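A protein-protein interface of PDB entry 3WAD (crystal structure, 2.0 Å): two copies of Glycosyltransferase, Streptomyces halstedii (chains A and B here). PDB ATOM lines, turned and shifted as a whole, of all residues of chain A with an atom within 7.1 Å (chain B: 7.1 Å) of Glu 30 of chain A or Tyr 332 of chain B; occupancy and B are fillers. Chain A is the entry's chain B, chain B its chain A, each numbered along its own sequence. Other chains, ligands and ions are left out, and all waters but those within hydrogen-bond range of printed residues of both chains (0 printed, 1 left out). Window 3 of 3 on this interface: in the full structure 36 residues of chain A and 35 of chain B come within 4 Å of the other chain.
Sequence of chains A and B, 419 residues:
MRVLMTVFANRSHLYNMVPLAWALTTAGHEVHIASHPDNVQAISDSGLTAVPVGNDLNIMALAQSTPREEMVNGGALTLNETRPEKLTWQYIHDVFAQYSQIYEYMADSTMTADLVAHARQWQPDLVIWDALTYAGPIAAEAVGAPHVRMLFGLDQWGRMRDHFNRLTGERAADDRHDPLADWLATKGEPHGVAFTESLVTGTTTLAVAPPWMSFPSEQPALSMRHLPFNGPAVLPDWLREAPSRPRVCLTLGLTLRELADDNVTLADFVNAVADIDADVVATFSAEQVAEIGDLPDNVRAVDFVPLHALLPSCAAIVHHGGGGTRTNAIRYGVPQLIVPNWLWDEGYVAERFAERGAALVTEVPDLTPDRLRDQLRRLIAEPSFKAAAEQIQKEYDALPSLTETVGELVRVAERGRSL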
ATOM      1  N   MET A   1      -7.636 -15.397  19.103  1.00  0.00           N
ATOM      2  CA  MET A   1      -7.900 -15.043  20.506  1.00  0.00           C
ATOM      3  C   MET A   1      -8.384 -16.309  21.191  1.00  0.00           C
ATOM      4  O   MET A   1      -8.738 -17.271  20.554  1.00  0.00           O
ATOM      5  CB  MET A   1      -8.998 -13.960  20.570  1.00  0.00           C
ATOM      6  CG  MET A   1     -10.323 -14.347  19.836  1.00  0.00           C
ATOM      7  SD  MET A   1     -11.628 -13.080  19.958  1.00  0.00           S
ATOM      8  CE  MET A   1     -11.130 -12.593  21.508  1.00  0.00           C
ATOM      9  N   ARG A   2      -8.351 -16.288  22.494  1.00  0.00           N
ATOM     10  CA  ARG A   2      -8.723 -17.421  23.304  1.00  0.00           C
ATOM     11  C   ARG A   2     -10.178 -17.125  23.800  1.00  0.00           C
ATOM     12  O   ARG A   2     -10.420 -16.028  24.386  1.00  0.00           O
ATOM     13  CB  ARG A   2      -7.790 -17.509  24.488  1.00  0.00           C
ATOM     14  CG  ARG A   2      -6.277 -17.528  24.057  1.00  0.00           C
ATOM     15  CD  ARG A   2      -5.512 -18.683  24.611  1.00  0.00           C
ATOM     16  NE  ARG A   2      -4.643 -18.407  25.743  1.00  0.00           N
ATOM     17  CZ  ARG A   2      -3.497 -19.066  26.045  1.00  0.00           C
ATOM     18  NH1 ARG A   2      -3.001 -20.056  25.295  1.00  0.00           N
ATOM     19  NH2 ARG A   2      -2.822 -18.733  27.117  1.00  0.00           N
ATOM     20  N   VAL A   3     -11.117 -18.053  23.513  1.00  0.00           N
ATOM     21  CA  VAL A   3     -12.510 -17.877  23.967  1.00  0.00           C
ATOM     22  C   VAL A   3     -12.851 -18.960  24.955  1.00  0.00           C
ATOM     23  O   VAL A   3     -12.804 -20.151  24.648  1.00  0.00           O
ATOM     24  CB  VAL A   3     -13.456 -17.980  22.811  1.00  0.00           C
ATOM     25  CG1 VAL A   3     -14.981 -17.621  23.273  1.00  0.00           C
ATOM     26  CG2 VAL A   3     -12.989 -17.122  21.653  1.00  0.00           C
ATOM     27  N   LEU A   4     -13.188 -18.567  26.145  1.00  0.00           N
ATOM     28  CA  LEU A   4     -13.653 -19.513  27.115  1.00  0.00           C
ATOM     29  C   LEU A   4     -15.212 -19.508  27.104  1.00  0.00           C
ATOM     30  O   LEU A   4     -15.849 -18.555  27.535  1.00  0.00           O
ATOM     31  CB  LEU A   4     -13.058 -19.184  28.495  1.00  0.00           C
ATOM     32  CG  LEU A   4     -13.490 -19.984  29.698  1.00  0.00           C
ATOM     33  CD1 LEU A   4     -13.133 -21.501  29.467  1.00  0.00           C
ATOM     34  CD2 LEU A   4     -12.932 -19.477  31.048  1.00  0.00           C
ATOM     35  N   LEU A  24     -16.261 -19.849  15.564  1.00  0.00           N
ATOM     36  CA  LEU A  24     -15.057 -19.307  16.180  1.00  0.00           C
ATOM     37  C   LEU A  24     -13.803 -20.177  15.921  1.00  0.00           C
ATOM     38  O   LEU A  24     -12.674 -19.652  15.648  1.00  0.00           O
ATOM     39  CB  LEU A  24     -15.267 -19.143  17.661  1.00  0.00           C
ATOM     40  CG  LEU A  24     -16.213 -17.989  18.092  1.00  0.00           C
ATOM     41  CD1 LEU A  24     -16.612 -18.249  19.567  1.00  0.00           C
ATOM     42  CD2 LEU A  24     -15.486 -16.539  17.986  1.00  0.00           C
ATOM     43  N   THR A  25     -13.980 -21.501  15.993  1.00  0.00           N
ATOM     44  CA  THR A  25     -12.856 -22.411  15.716  1.00  0.00           C
ATOM     45  C   THR A  25     -12.343 -22.279  14.265  1.00  0.00           C
ATOM     46  O   THR A  25     -11.141 -22.209  14.042  1.00  0.00           O
ATOM     47  CB  THR A  25     -13.266 -23.858  16.070  1.00  0.00           C
ATOM     48  OG1 THR A  25     -13.619 -23.885  17.477  1.00  0.00           O
ATOM     49  CG2 THR A  25     -12.112 -24.848  15.841  1.00  0.00           C
ATOM     50  N   GLY A  28     -10.249 -19.388  13.466  1.00  0.00           N
ATOM     51  CA  GLY A  28      -8.824 -19.559  13.893  1.00  0.00           C
ATOM     52  C   GLY A  28      -8.622 -19.387  15.381  1.00  0.00           C
ATOM     53  O   GLY A  28      -7.494 -19.531  15.948  1.00  0.00           O
ATOM     54  N   HIS A  29      -9.718 -19.089  16.070  1.00  0.00           N
ATOM     55  CA  HIS A  29      -9.586 -18.860  17.458  1.00  0.00           C
ATOM     56  C   HIS A  29      -9.505 -20.172  18.178  1.00  0.00           C
ATOM     57  O   HIS A  29      -9.955 -21.182  17.631  1.00  0.00           O
ATOM     58  CB  HIS A  29     -10.781 -18.033  17.853  1.00  0.00           C
ATOM     59  CG  HIS A  29     -10.946 -16.828  16.972  1.00  0.00           C
ATOM     60  ND1 HIS A  29     -10.081 -15.749  17.034  1.00  0.00           N
ATOM     61  CD2 HIS A  29     -11.829 -16.555  15.973  1.00  0.00           C
ATOM     62  CE1 HIS A  29     -10.438 -14.857  16.125  1.00  0.00           C
ATOM     63  NE2 HIS A  29     -11.505 -15.310  15.481  1.00  0.00           N
ATOM     64  N   GLU A  30      -8.998 -20.153  19.415  1.00  0.00           N
ATOM     65  CA  GLU A  30      -8.855 -21.323  20.271  1.00  0.00           C
ATOM     66  C   GLU A  30     -10.050 -21.303  21.235  1.00  0.00           C
ATOM     67  O   GLU A  30     -10.201 -20.345  22.014  1.00  0.00           O
ATOM     68  CB  GLU A  30      -7.636 -21.233  21.175  1.00  0.00           C
ATOM     69  CG  GLU A  30      -6.327 -21.067  20.479  1.00  0.00           C
ATOM     70  CD  GLU A  30      -5.759 -22.389  20.033  1.00  0.00           C
ATOM     71  OE1 GLU A  30      -5.367 -22.491  18.844  1.00  0.00           O
ATOM     72  OE2 GLU A  30      -5.724 -23.336  20.859  1.00  0.00           O
ATOM     73  N   VAL A  31     -10.876 -22.343  21.187  1.00  0.00           N
ATOM     74  CA  VAL A  31     -12.142 -22.344  21.957  1.00  0.00           C
ATOM     75  C   VAL A  31     -12.096 -23.493  22.952  1.00  0.00           C
ATOM     76  O   VAL A  31     -11.806 -24.622  22.586  1.00  0.00           O
ATOM     77  CB  VAL A  31     -13.274 -22.561  20.995  1.00  0.00           C
ATOM     78  CG1 VAL A  31     -14.639 -22.575  21.721  1.00  0.00           C
ATOM     79  CG2 VAL A  31     -13.261 -21.446  19.912  1.00  0.00           C
ATOM     80  N   HIS A  32     -12.291 -23.177  24.212  1.00  0.00           N
ATOM     81  CA  HIS A  32     -12.495 -24.162  25.244  1.00  0.00           C
ATOM     82  C   HIS A  32     -13.983 -24.184  25.672  1.00  0.00           C
ATOM     83  O   HIS A  32     -14.578 -23.100  25.961  1.00  0.00           O
ATOM     84  CB  HIS A  32     -11.611 -23.862  26.485  1.00  0.00           C
ATOM     85  CG  HIS A  32     -10.148 -24.152  26.283  1.00  0.00           C
ATOM     86  ND1 HIS A  32      -9.189 -23.778  27.199  1.00  0.00           N
ATOM     87  CD2 HIS A  32      -9.484 -24.781  25.288  1.00  0.00           C
ATOM     88  CE1 HIS A  32      -8.004 -24.191  26.789  1.00  0.00           C
ATOM     89  NE2 HIS A  32      -8.150 -24.768  25.616  1.00  0.00           N
ATOM     90  N   TRP A 122      -5.401 -19.774  31.804  1.00  0.00           N
ATOM     91  CA  TRP A 122      -5.506 -19.645  30.335  1.00  0.00           C
ATOM     92  C   TRP A 122      -5.591 -18.233  29.856  1.00  0.00           C
ATOM     93  O   TRP A 122      -5.422 -17.940  28.624  1.00  0.00           O
ATOM     94  CB  TRP A 122      -6.807 -20.348  29.819  1.00  0.00           C
ATOM     95  CG  TRP A 122      -6.782 -20.698  28.322  1.00  0.00           C
ATOM     96  CD1 TRP A 122      -5.702 -21.258  27.657  1.00  0.00           C
ATOM     97  CD2 TRP A 122      -7.847 -20.640  27.348  1.00  0.00           C
ATOM     98  NE1 TRP A 122      -6.008 -21.509  26.384  1.00  0.00           N
ATOM     99  CE2 TRP A 122      -7.314 -21.145  26.134  1.00  0.00           C
ATOM    100  CE3 TRP A 122      -9.189 -20.239  27.378  1.00  0.00           C
ATOM    101  CZ2 TRP A 122      -8.080 -21.254  24.939  1.00  0.00           C
ATOM    102  CZ3 TRP A 122      -9.945 -20.324  26.200  1.00  0.00           C
ATOM    103  CH2 TRP A 122      -9.383 -20.813  24.977  1.00  0.00           C
ATOM    104  N   LEU B 227      -6.409 -26.484   9.768  1.00  0.00           N
ATOM    105  CA  LEU B 227      -6.775 -26.781  11.149  1.00  0.00           C
ATOM    106  C   LEU B 227      -6.697 -28.319  11.427  1.00  0.00           C
ATOM    107  O   LEU B 227      -7.405 -29.110  10.744  1.00  0.00           O
ATOM    108  CB  LEU B 227      -8.194 -26.264  11.386  1.00  0.00           C
ATOM    109  CG  LEU B 227      -8.376 -24.857  11.972  1.00  0.00           C
ATOM    110  CD1 LEU B 227      -9.808 -24.676  12.434  1.00  0.00           C
ATOM    111  CD2 LEU B 227      -7.450 -24.622  13.153  1.00  0.00           C
ATOM    112  N   PRO B 228      -5.797 -28.744  12.362  1.00  0.00           N
ATOM    113  CA  PRO B 228      -5.629 -30.177  12.644  1.00  0.00           C
ATOM    114  C   PRO B 228      -6.705 -30.627  13.640  1.00  0.00           C
ATOM    115  O   PRO B 228      -6.873 -29.979  14.641  1.00  0.00           O
ATOM    116  CB  PRO B 228      -4.238 -30.284  13.312  1.00  0.00           C
ATOM    117  CG  PRO B 228      -3.920 -28.882  13.849  1.00  0.00           C
ATOM    118  CD  PRO B 228      -4.956 -27.897  13.241  1.00  0.00           C
ATOM    119  N   LEU B 307      -3.180 -32.580  21.571  1.00  0.00           N
ATOM    120  CA  LEU B 307      -1.926 -31.952  21.238  1.00  0.00           C
ATOM    121  C   LEU B 307      -2.093 -30.465  21.210  1.00  0.00           C
ATOM    122  O   LEU B 307      -1.241 -29.743  21.690  1.00  0.00           O
ATOM    123  CB  LEU B 307      -1.462 -32.433  19.877  1.00  0.00           C
ATOM    124  CG  LEU B 307      -0.241 -33.335  19.764  1.00  0.00           C
ATOM    125  CD1 LEU B 307       0.303 -33.860  21.071  1.00  0.00           C
ATOM    126  CD2 LEU B 307      -0.603 -34.424  18.806  1.00  0.00           C
ATOM    127  N   HIS B 308      -3.222 -30.012  20.666  1.00  0.00           N
ATOM    128  CA  HIS B 308      -3.476 -28.578  20.564  1.00  0.00           C
ATOM    129  C   HIS B 308      -3.550 -27.858  21.948  1.00  0.00           C
ATOM    130  O   HIS B 308      -3.348 -26.657  22.013  1.00  0.00           O
ATOM    131  CB  HIS B 308      -4.712 -28.293  19.689  1.00  0.00           C
ATOM    132  CG  HIS B 308      -5.968 -28.935  20.216  1.00  0.00           C
ATOM    133  ND1 HIS B 308      -6.818 -28.300  21.092  1.00  0.00           N
ATOM    134  CD2 HIS B 308      -6.465 -30.180  20.053  1.00  0.00           C
ATOM    135  CE1 HIS B 308      -7.818 -29.109  21.400  1.00  0.00           C
ATOM    136  NE2 HIS B 308      -7.625 -30.256  20.783  1.00  0.00           N
ATOM    137  N   ALA B 309      -3.774 -28.581  23.045  1.00  0.00           N
ATOM    138  CA  ALA B 309      -3.764 -27.982  24.376  1.00  0.00           C
ATOM    139  C   ALA B 309      -2.451 -28.197  25.114  1.00  0.00           C
ATOM    140  O   ALA B 309      -2.134 -27.414  26.002  1.00  0.00           O
ATOM    141  CB  ALA B 309      -4.916 -28.555  25.244  1.00  0.00           C
ATOM    142  N   LEU B 310      -1.702 -29.262  24.785  1.00  0.00           N
ATOM    143  CA  LEU B 310      -0.394 -29.452  25.408  1.00  0.00           C
ATOM    144  C   LEU B 310       0.717 -28.557  24.773  1.00  0.00           C
ATOM    145  O   LEU B 310       1.522 -27.992  25.481  1.00  0.00           O
ATOM    146  CB  LEU B 310       0.006 -30.908  25.320  1.00  0.00           C
ATOM    147  CG  LEU B 310       1.407 -31.357  25.678  1.00  0.00           C
ATOM    148  CD1 LEU B 310       1.767 -31.002  27.126  1.00  0.00           C
ATOM    149  CD2 LEU B 310       1.395 -32.854  25.438  1.00  0.00           C
ATOM    150  N   LEU B 311       0.736 -28.464  23.448  1.00  0.00           N
ATOM    151  CA  LEU B 311       1.880 -27.867  22.741  1.00  0.00           C
ATOM    152  C   LEU B 311       2.234 -26.412  23.069  1.00  0.00           C
ATOM    153  O   LEU B 311       3.416 -26.069  23.041  1.00  0.00           O
ATOM    154  CB  LEU B 311       1.768 -28.081  21.236  1.00  0.00           C
ATOM    155  CG  LEU B 311       2.053 -29.500  20.722  1.00  0.00           C
ATOM    156  CD1 LEU B 311       1.959 -29.533  19.274  1.00  0.00           C
ATOM    157  CD2 LEU B 311       3.474 -29.925  21.098  1.00  0.00           C
ATOM    158  N   PRO B 312       1.231 -25.558  23.393  1.00  0.00           N
ATOM    159  CA  PRO B 312       1.531 -24.178  23.831  1.00  0.00           C
ATOM    160  C   PRO B 312       2.514 -24.072  24.951  1.00  0.00           C
ATOM    161  O   PRO B 312       3.147 -23.021  25.080  1.00  0.00           O
ATOM    162  CB  PRO B 312       0.168 -23.630  24.273  1.00  0.00           C
ATOM    163  CG  PRO B 312      -0.808 -24.307  23.295  1.00  0.00           C
ATOM    164  CD  PRO B 312      -0.212 -25.740  23.149  1.00  0.00           C
ATOM    165  N   SER B 313       2.678 -25.131  25.740  1.00  0.00           N
ATOM    166  CA  SER B 313       3.623 -25.071  26.841  1.00  0.00           C
ATOM    167  C   SER B 313       4.872 -25.922  26.617  1.00  0.00           C
ATOM    168  O   SER B 313       5.660 -26.125  27.559  1.00  0.00           O
ATOM    169  CB  SER B 313       2.930 -25.486  28.164  1.00  0.00           C
ATOM    170  OG  SER B 313       2.564 -26.873  28.149  1.00  0.00           O
ATOM    171  N   CYS B 314       5.066 -26.403  25.393  1.00  0.00           N
ATOM    172  CA  CYS B 314       6.143 -27.350  25.045  1.00  0.00           C
ATOM    173  C   CYS B 314       7.305 -26.732  24.248  1.00  0.00           C
ATOM    174  O   CYS B 314       7.111 -25.882  23.421  1.00  0.00           O
ATOM    175  CB  CYS B 314       5.586 -28.504  24.213  1.00  0.00           C
ATOM    176  SG  CYS B 314       4.488 -29.619  25.172  1.00  0.00           S
ATOM    177  N   ARG B 326       2.403 -32.653  12.974  1.00  0.00           N
ATOM    178  CA  ARG B 326       3.244 -31.606  12.376  1.00  0.00           C
ATOM    179  C   ARG B 326       2.439 -30.318  12.139  1.00  0.00           C
ATOM    180  O   ARG B 326       2.983 -29.269  12.300  1.00  0.00           O
ATOM    181  CB  ARG B 326       3.975 -32.052  11.107  1.00  0.00           C
ATOM    182  CG  ARG B 326       3.123 -32.138   9.857  1.00  0.00           C
ATOM    183  CD  ARG B 326       3.855 -33.032   8.839  1.00  0.00           C
ATOM    184  NE  ARG B 326       3.163 -32.957   7.558  1.00  0.00           N
ATOM    185  CZ  ARG B 326       3.192 -33.893   6.630  1.00  0.00           C
ATOM    186  NH1 ARG B 326       3.941 -34.983   6.778  1.00  0.00           N
ATOM    187  NH2 ARG B 326       2.492 -33.704   5.533  1.00  0.00           N
ATOM    188  N   THR B 327       1.146 -30.405  11.825  1.00  0.00           N
ATOM    189  CA  THR B 327       0.325 -29.200  11.624  1.00  0.00           C
ATOM    190  C   THR B 327       0.192 -28.504  12.961  1.00  0.00           C
ATOM    191  O   THR B 327       0.271 -27.269  13.023  1.00  0.00           O
ATOM    192  CB  THR B 327      -1.004 -29.521  11.040  1.00  0.00           C
ATOM    193  OG1 THR B 327      -0.771 -30.087   9.772  1.00  0.00           O
ATOM    194  CG2 THR B 327      -1.832 -28.279  10.837  1.00  0.00           C
ATOM    195  N   ASN B 328       0.089 -29.303  14.029  1.00  0.00           N
ATOM    196  CA  ASN B 328       0.142 -28.744  15.379  1.00  0.00           C
ATOM    197  C   ASN B 328       1.474 -28.014  15.704  1.00  0.00           C
ATOM    198  O   ASN B 328       1.482 -26.939  16.317  1.00  0.00           O
ATOM    199  CB  ASN B 328      -0.205 -29.814  16.424  1.00  0.00           C
ATOM    200  CG  ASN B 328      -1.726 -30.001  16.600  1.00  0.00           C
ATOM    201  OD1 ASN B 328      -2.366 -29.135  17.183  1.00  0.00           O
ATOM    202  ND2 ASN B 328      -2.294 -31.143  16.111  1.00  0.00           N
ATOM    203  N   ALA B 329       2.591 -28.630  15.322  1.00  0.00           N
ATOM    204  CA  ALA B 329       3.901 -28.042  15.544  1.00  0.00           C
ATOM    205  C   ALA B 329       4.031 -26.728  14.788  1.00  0.00           C
ATOM    206  O   ALA B 329       4.591 -25.787  15.316  1.00  0.00           O
ATOM    207  CB  ALA B 329       5.059 -29.040  15.149  1.00  0.00           C
ATOM    208  N   ILE B 330       3.509 -26.688  13.580  1.00  0.00           N
ATOM    209  CA  ILE B 330       3.487 -25.457  12.759  1.00  0.00           C
ATOM    210  C   ILE B 330       2.662 -24.379  13.477  1.00  0.00           C
ATOM    211  O   ILE B 330       3.126 -23.213  13.706  1.00  0.00           O
ATOM    212  CB  ILE B 330       2.904 -25.783  11.353  1.00  0.00           C
ATOM    213  CG1 ILE B 330       3.870 -26.699  10.558  1.00  0.00           C
ATOM    214  CG2 ILE B 330       2.640 -24.497  10.529  1.00  0.00           C
ATOM    215  CD1 ILE B 330       3.277 -27.220   9.246  1.00  0.00           C
ATOM    216  N   ARG B 331       1.469 -24.785  13.915  1.00  0.00           N
ATOM    217  CA  ARG B 331       0.481 -23.855  14.449  1.00  0.00           C
ATOM    218  C   ARG B 331       0.883 -23.222  15.753  1.00  0.00           C
ATOM    219  O   ARG B 331       0.575 -22.048  15.969  1.00  0.00           O
ATOM    220  CB  ARG B 331      -0.851 -24.538  14.568  1.00  0.00           C
ATOM    221  CG  ARG B 331      -1.893 -23.632  15.043  1.00  0.00           C
ATOM    222  CD  ARG B 331      -3.161 -24.474  15.403  1.00  0.00           C
ATOM    223  NE  ARG B 331      -4.157 -23.438  15.589  1.00  0.00           N
ATOM    224  CZ  ARG B 331      -5.419 -23.662  15.846  1.00  0.00           C
ATOM    225  NH1 ARG B 331      -5.845 -24.931  16.013  1.00  0.00           N
ATOM    226  NH2 ARG B 331      -6.229 -22.628  15.950  1.00  0.00           N
ATOM    227  N   TYR B 332       1.607 -23.960  16.599  1.00  0.00           N
ATOM    228  CA  TYR B 332       2.079 -23.471  17.892  1.00  0.00           C
ATOM    229  C   TYR B 332       3.565 -23.191  17.840  1.00  0.00           C
ATOM    230  O   TYR B 332       4.191 -22.905  18.820  1.00  0.00           O
ATOM    231  CB  TYR B 332       1.729 -24.486  19.024  1.00  0.00           C
ATOM    232  CG  TYR B 332       0.228 -24.629  19.072  1.00  0.00           C
ATOM    233  CD1 TYR B 332      -0.591 -23.590  19.526  1.00  0.00           C
ATOM    234  CD2 TYR B 332      -0.371 -25.763  18.553  1.00  0.00           C
ATOM    235  CE1 TYR B 332      -2.012 -23.705  19.505  1.00  0.00           C
ATOM    236  CE2 TYR B 332      -1.767 -25.900  18.563  1.00  0.00           C
ATOM    237  CZ  TYR B 332      -2.554 -24.880  19.050  1.00  0.00           C
ATOM    238  OH  TYR B 332      -3.875 -25.087  18.976  1.00  0.00           O
ATOM    239  N   GLY B 333       4.135 -23.176  16.633  1.00  0.00           N
ATOM    240  CA  GLY B 333       5.565 -22.837  16.584  1.00  0.00           C
ATOM    241  C   GLY B 333       6.476 -23.687  17.474  1.00  0.00           C
ATOM    242  O   GLY B 333       7.371 -23.145  18.060  1.00  0.00           O
ATOM    243  N   VAL B 334       6.341 -25.013  17.440  1.00  0.00           N
ATOM    244  CA  VAL B 334       7.142 -25.878  18.300  1.00  0.00           C
ATOM    245  C   VAL B 334       8.211 -26.627  17.468  1.00  0.00           C
ATOM    246  O   VAL B 334       7.891 -27.269  16.448  1.00  0.00           O
ATOM    247  CB  VAL B 334       6.257 -26.916  19.075  1.00  0.00           C
ATOM    248  CG1 VAL B 334       7.097 -27.831  19.888  1.00  0.00           C
ATOM    249  CG2 VAL B 334       5.231 -26.213  19.980  1.00  0.00           C
ATOM    250  N   PRO B 335       9.476 -26.567  17.935  1.00  0.00           N
ATOM    251  CA  PRO B 335      10.559 -27.359  17.313  1.00  0.00           C
ATOM    252  C   PRO B 335      10.290 -28.875  17.415  1.00  0.00           C
ATOM    253  O   PRO B 335       9.594 -29.334  18.367  1.00  0.00           O
ATOM    254  CB  PRO B 335      11.800 -26.915  18.069  1.00  0.00           C
ATOM    255  CG  PRO B 335      11.383 -25.786  18.974  1.00  0.00           C
ATOM    256  CD  PRO B 335       9.938 -25.561  18.917  1.00  0.00           C
ATOM    257  N   LYS B 386      13.630 -22.880  18.029  1.00  0.00           N
ATOM    258  CA  LYS B 386      12.400 -22.137  18.391  1.00  0.00           C
ATOM    259  C   LYS B 386      12.198 -20.935  17.453  1.00  0.00           C
ATOM    260  O   LYS B 386      11.069 -20.690  16.972  1.00  0.00           O
ATOM    261  CB  LYS B 386      12.428 -21.762  19.898  1.00  0.00           C
ATOM    262  CG  LYS B 386      11.234 -20.942  20.402  1.00  0.00           C
ATOM    263  CD  LYS B 386       9.934 -21.791  20.365  1.00  0.00           C
ATOM    264  CE  LYS B 386       8.673 -20.902  20.579  1.00  0.00           C
ATOM    265  NZ  LYS B 386       7.422 -21.765  20.577  1.00  0.00           N
ATOM    266  N   ALA B 389      11.053 -22.435  14.143  1.00  0.00           N
ATOM    267  CA  ALA B 389       9.653 -22.925  14.363  1.00  0.00           C
ATOM    268  C   ALA B 389       8.671 -21.732  14.328  1.00  0.00           C
ATOM    269  O   ALA B 389       7.611 -21.781  13.667  1.00  0.00           O
ATOM    270  CB  ALA B 389       9.533 -23.699  15.719  1.00  0.00           C
ATOM    271  N   GLU B 390       9.055 -20.617  14.978  1.00  0.00           N
ATOM    272  CA  GLU B 390       8.150 -19.444  15.051  1.00  0.00           C
ATOM    273  C   GLU B 390       7.979 -18.714  13.766  1.00  0.00           C
ATOM    274  O   GLU B 390       6.925 -18.162  13.538  1.00  0.00           O
ATOM    275  CB  GLU B 390       8.588 -18.448  16.120  1.00  0.00           C
ATOM    276  CG  GLU B 390       8.444 -18.957  17.516  1.00  0.00           C
ATOM    277  CD  GLU B 390       8.402 -17.790  18.447  1.00  0.00           C
ATOM    278  OE1 GLU B 390       9.154 -17.726  19.448  1.00  0.00           O
ATOM    279  OE2 GLU B 390       7.599 -16.888  18.136  1.00  0.00           O
ATOM    280  N   GLN B 393       5.417 -20.699  11.798  1.00  0.00           N
ATOM    281  CA  GLN B 393       4.108 -20.349  12.353  1.00  0.00           C
ATOM    282  C   GLN B 393       3.561 -19.002  11.820  1.00  0.00           C
ATOM    283  O   GLN B 393       2.385 -18.882  11.457  1.00  0.00           O
ATOM    284  CB  GLN B 393       4.293 -20.254  13.850  1.00  0.00           C
ATOM    285  CG  GLN B 393       3.024 -19.846  14.683  1.00  0.00           C
ATOM    286  CD  GLN B 393       3.378 -19.632  16.141  1.00  0.00           C
ATOM    287  OE1 GLN B 393       4.449 -19.105  16.457  1.00  0.00           O
ATOM    288  NE2 GLN B 393       2.499 -20.050  17.044  1.00  0.00           N
ATOM    289  N   TYR B 396       2.429 -19.637   8.458  1.00  0.00           N
ATOM    290  CA  TYR B 396       1.181 -20.424   8.485  1.00  0.00           C
ATOM    291  C   TYR B 396       0.000 -19.468   8.765  1.00  0.00           C
ATOM    292  O   TYR B 396      -1.025 -19.503   8.076  1.00  0.00           O
ATOM    293  CB  TYR B 396       1.328 -21.459   9.616  1.00  0.00           C
ATOM    294  CG  TYR B 396       0.026 -22.054  10.108  1.00  0.00           C
ATOM    295  CD1 TYR B 396      -0.575 -23.107   9.417  1.00  0.00           C
ATOM    296  CD2 TYR B 396      -0.583 -21.572  11.236  1.00  0.00           C
ATOM    297  CE1 TYR B 396      -1.802 -23.679   9.877  1.00  0.00           C
ATOM    298  CE2 TYR B 396      -1.802 -22.121  11.711  1.00  0.00           C
ATOM    299  CZ  TYR B 396      -2.360 -23.179  11.052  1.00  0.00           C
ATOM    300  OH  TYR B 396      -3.538 -23.707  11.499  1.00  0.00           O
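Hydrophobic or aromatic side chains of chain B that line the printed part of chain A: Leu 227 and Tyr 332. Of the 12 printed residues of chain A, 3 touch a printed residue of chain B. Printed residues of chain A that touch a printed residue of chain B: Thr 25, Gly 28 and Glu 30. Among the printed residues, Asp or Glu carboxylates within 4 Å of a Lys or Arg side-chain nitrogen of the other chain: Glu 30 of chain A with Arg 331 of chain B (3.0 Å).
Among the printed residues, pairs that only touch across the chains: Thr 25 of chain A with Leu 227 of chain B.
OH of Tyr 332 of chain B sits at hydrogen-bond distance from OE1 of Glu 30 of chain A (3.0 Å). O of Gly 28 of chain A lies within hydrogen-bond range of NH2 of Arg 331 of chain B (3.3 Å). NH2 of Arg 331 of chain B is in salt-bridge range of OE1 of Glu 30 of chain A, at 3.0 Å.
The backbone carbonyl oxygen of Arg 331 of chain B is in hydrogen-bond range of the side-chain amide nitrogen of Gln 393 of chain B, at 3.0 Å. The backbone NH of Glu 30 of chain A is in hydrogen-bond range of the backbone carbonyl oxygen of Met 1 of chain A (3.1 Å). O of Glu 30 of chain A lies within hydrogen-bond range of N of Val 3 of chain A (2.9 Å). The backbone carbonyl oxygen (O) of His 308 of chain B lies close to the side-chain hydroxyl (OH) of Tyr 332 of chain B (3.5 Å).
Of the printed residues of chain B, Thr 25 of chain A touches Leu 227 (3.2 Å). Of the printed residues of chain B, Gly 28 of chain A touches Arg 331. Of the printed residues of chain A, Leu 227 of chain B touches Thr 25 (3.2 Å). Leu 311 of chain B touches none of the printed residues of chain A. Of the printed residues of chain A, Arg 331 of chain B touches Gly 28 and Glu 30. Of chain A, only Glu 30 (3.0 Å) comes within 4 Å of Tyr 332 of chain B. Gly 333 of chain B touches none of the printed residues of chain A.
No position is printed for both chains. Of the 4 pairs that touch across the chains among the printed residues, none has its exchanged pair printed and touching as well.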
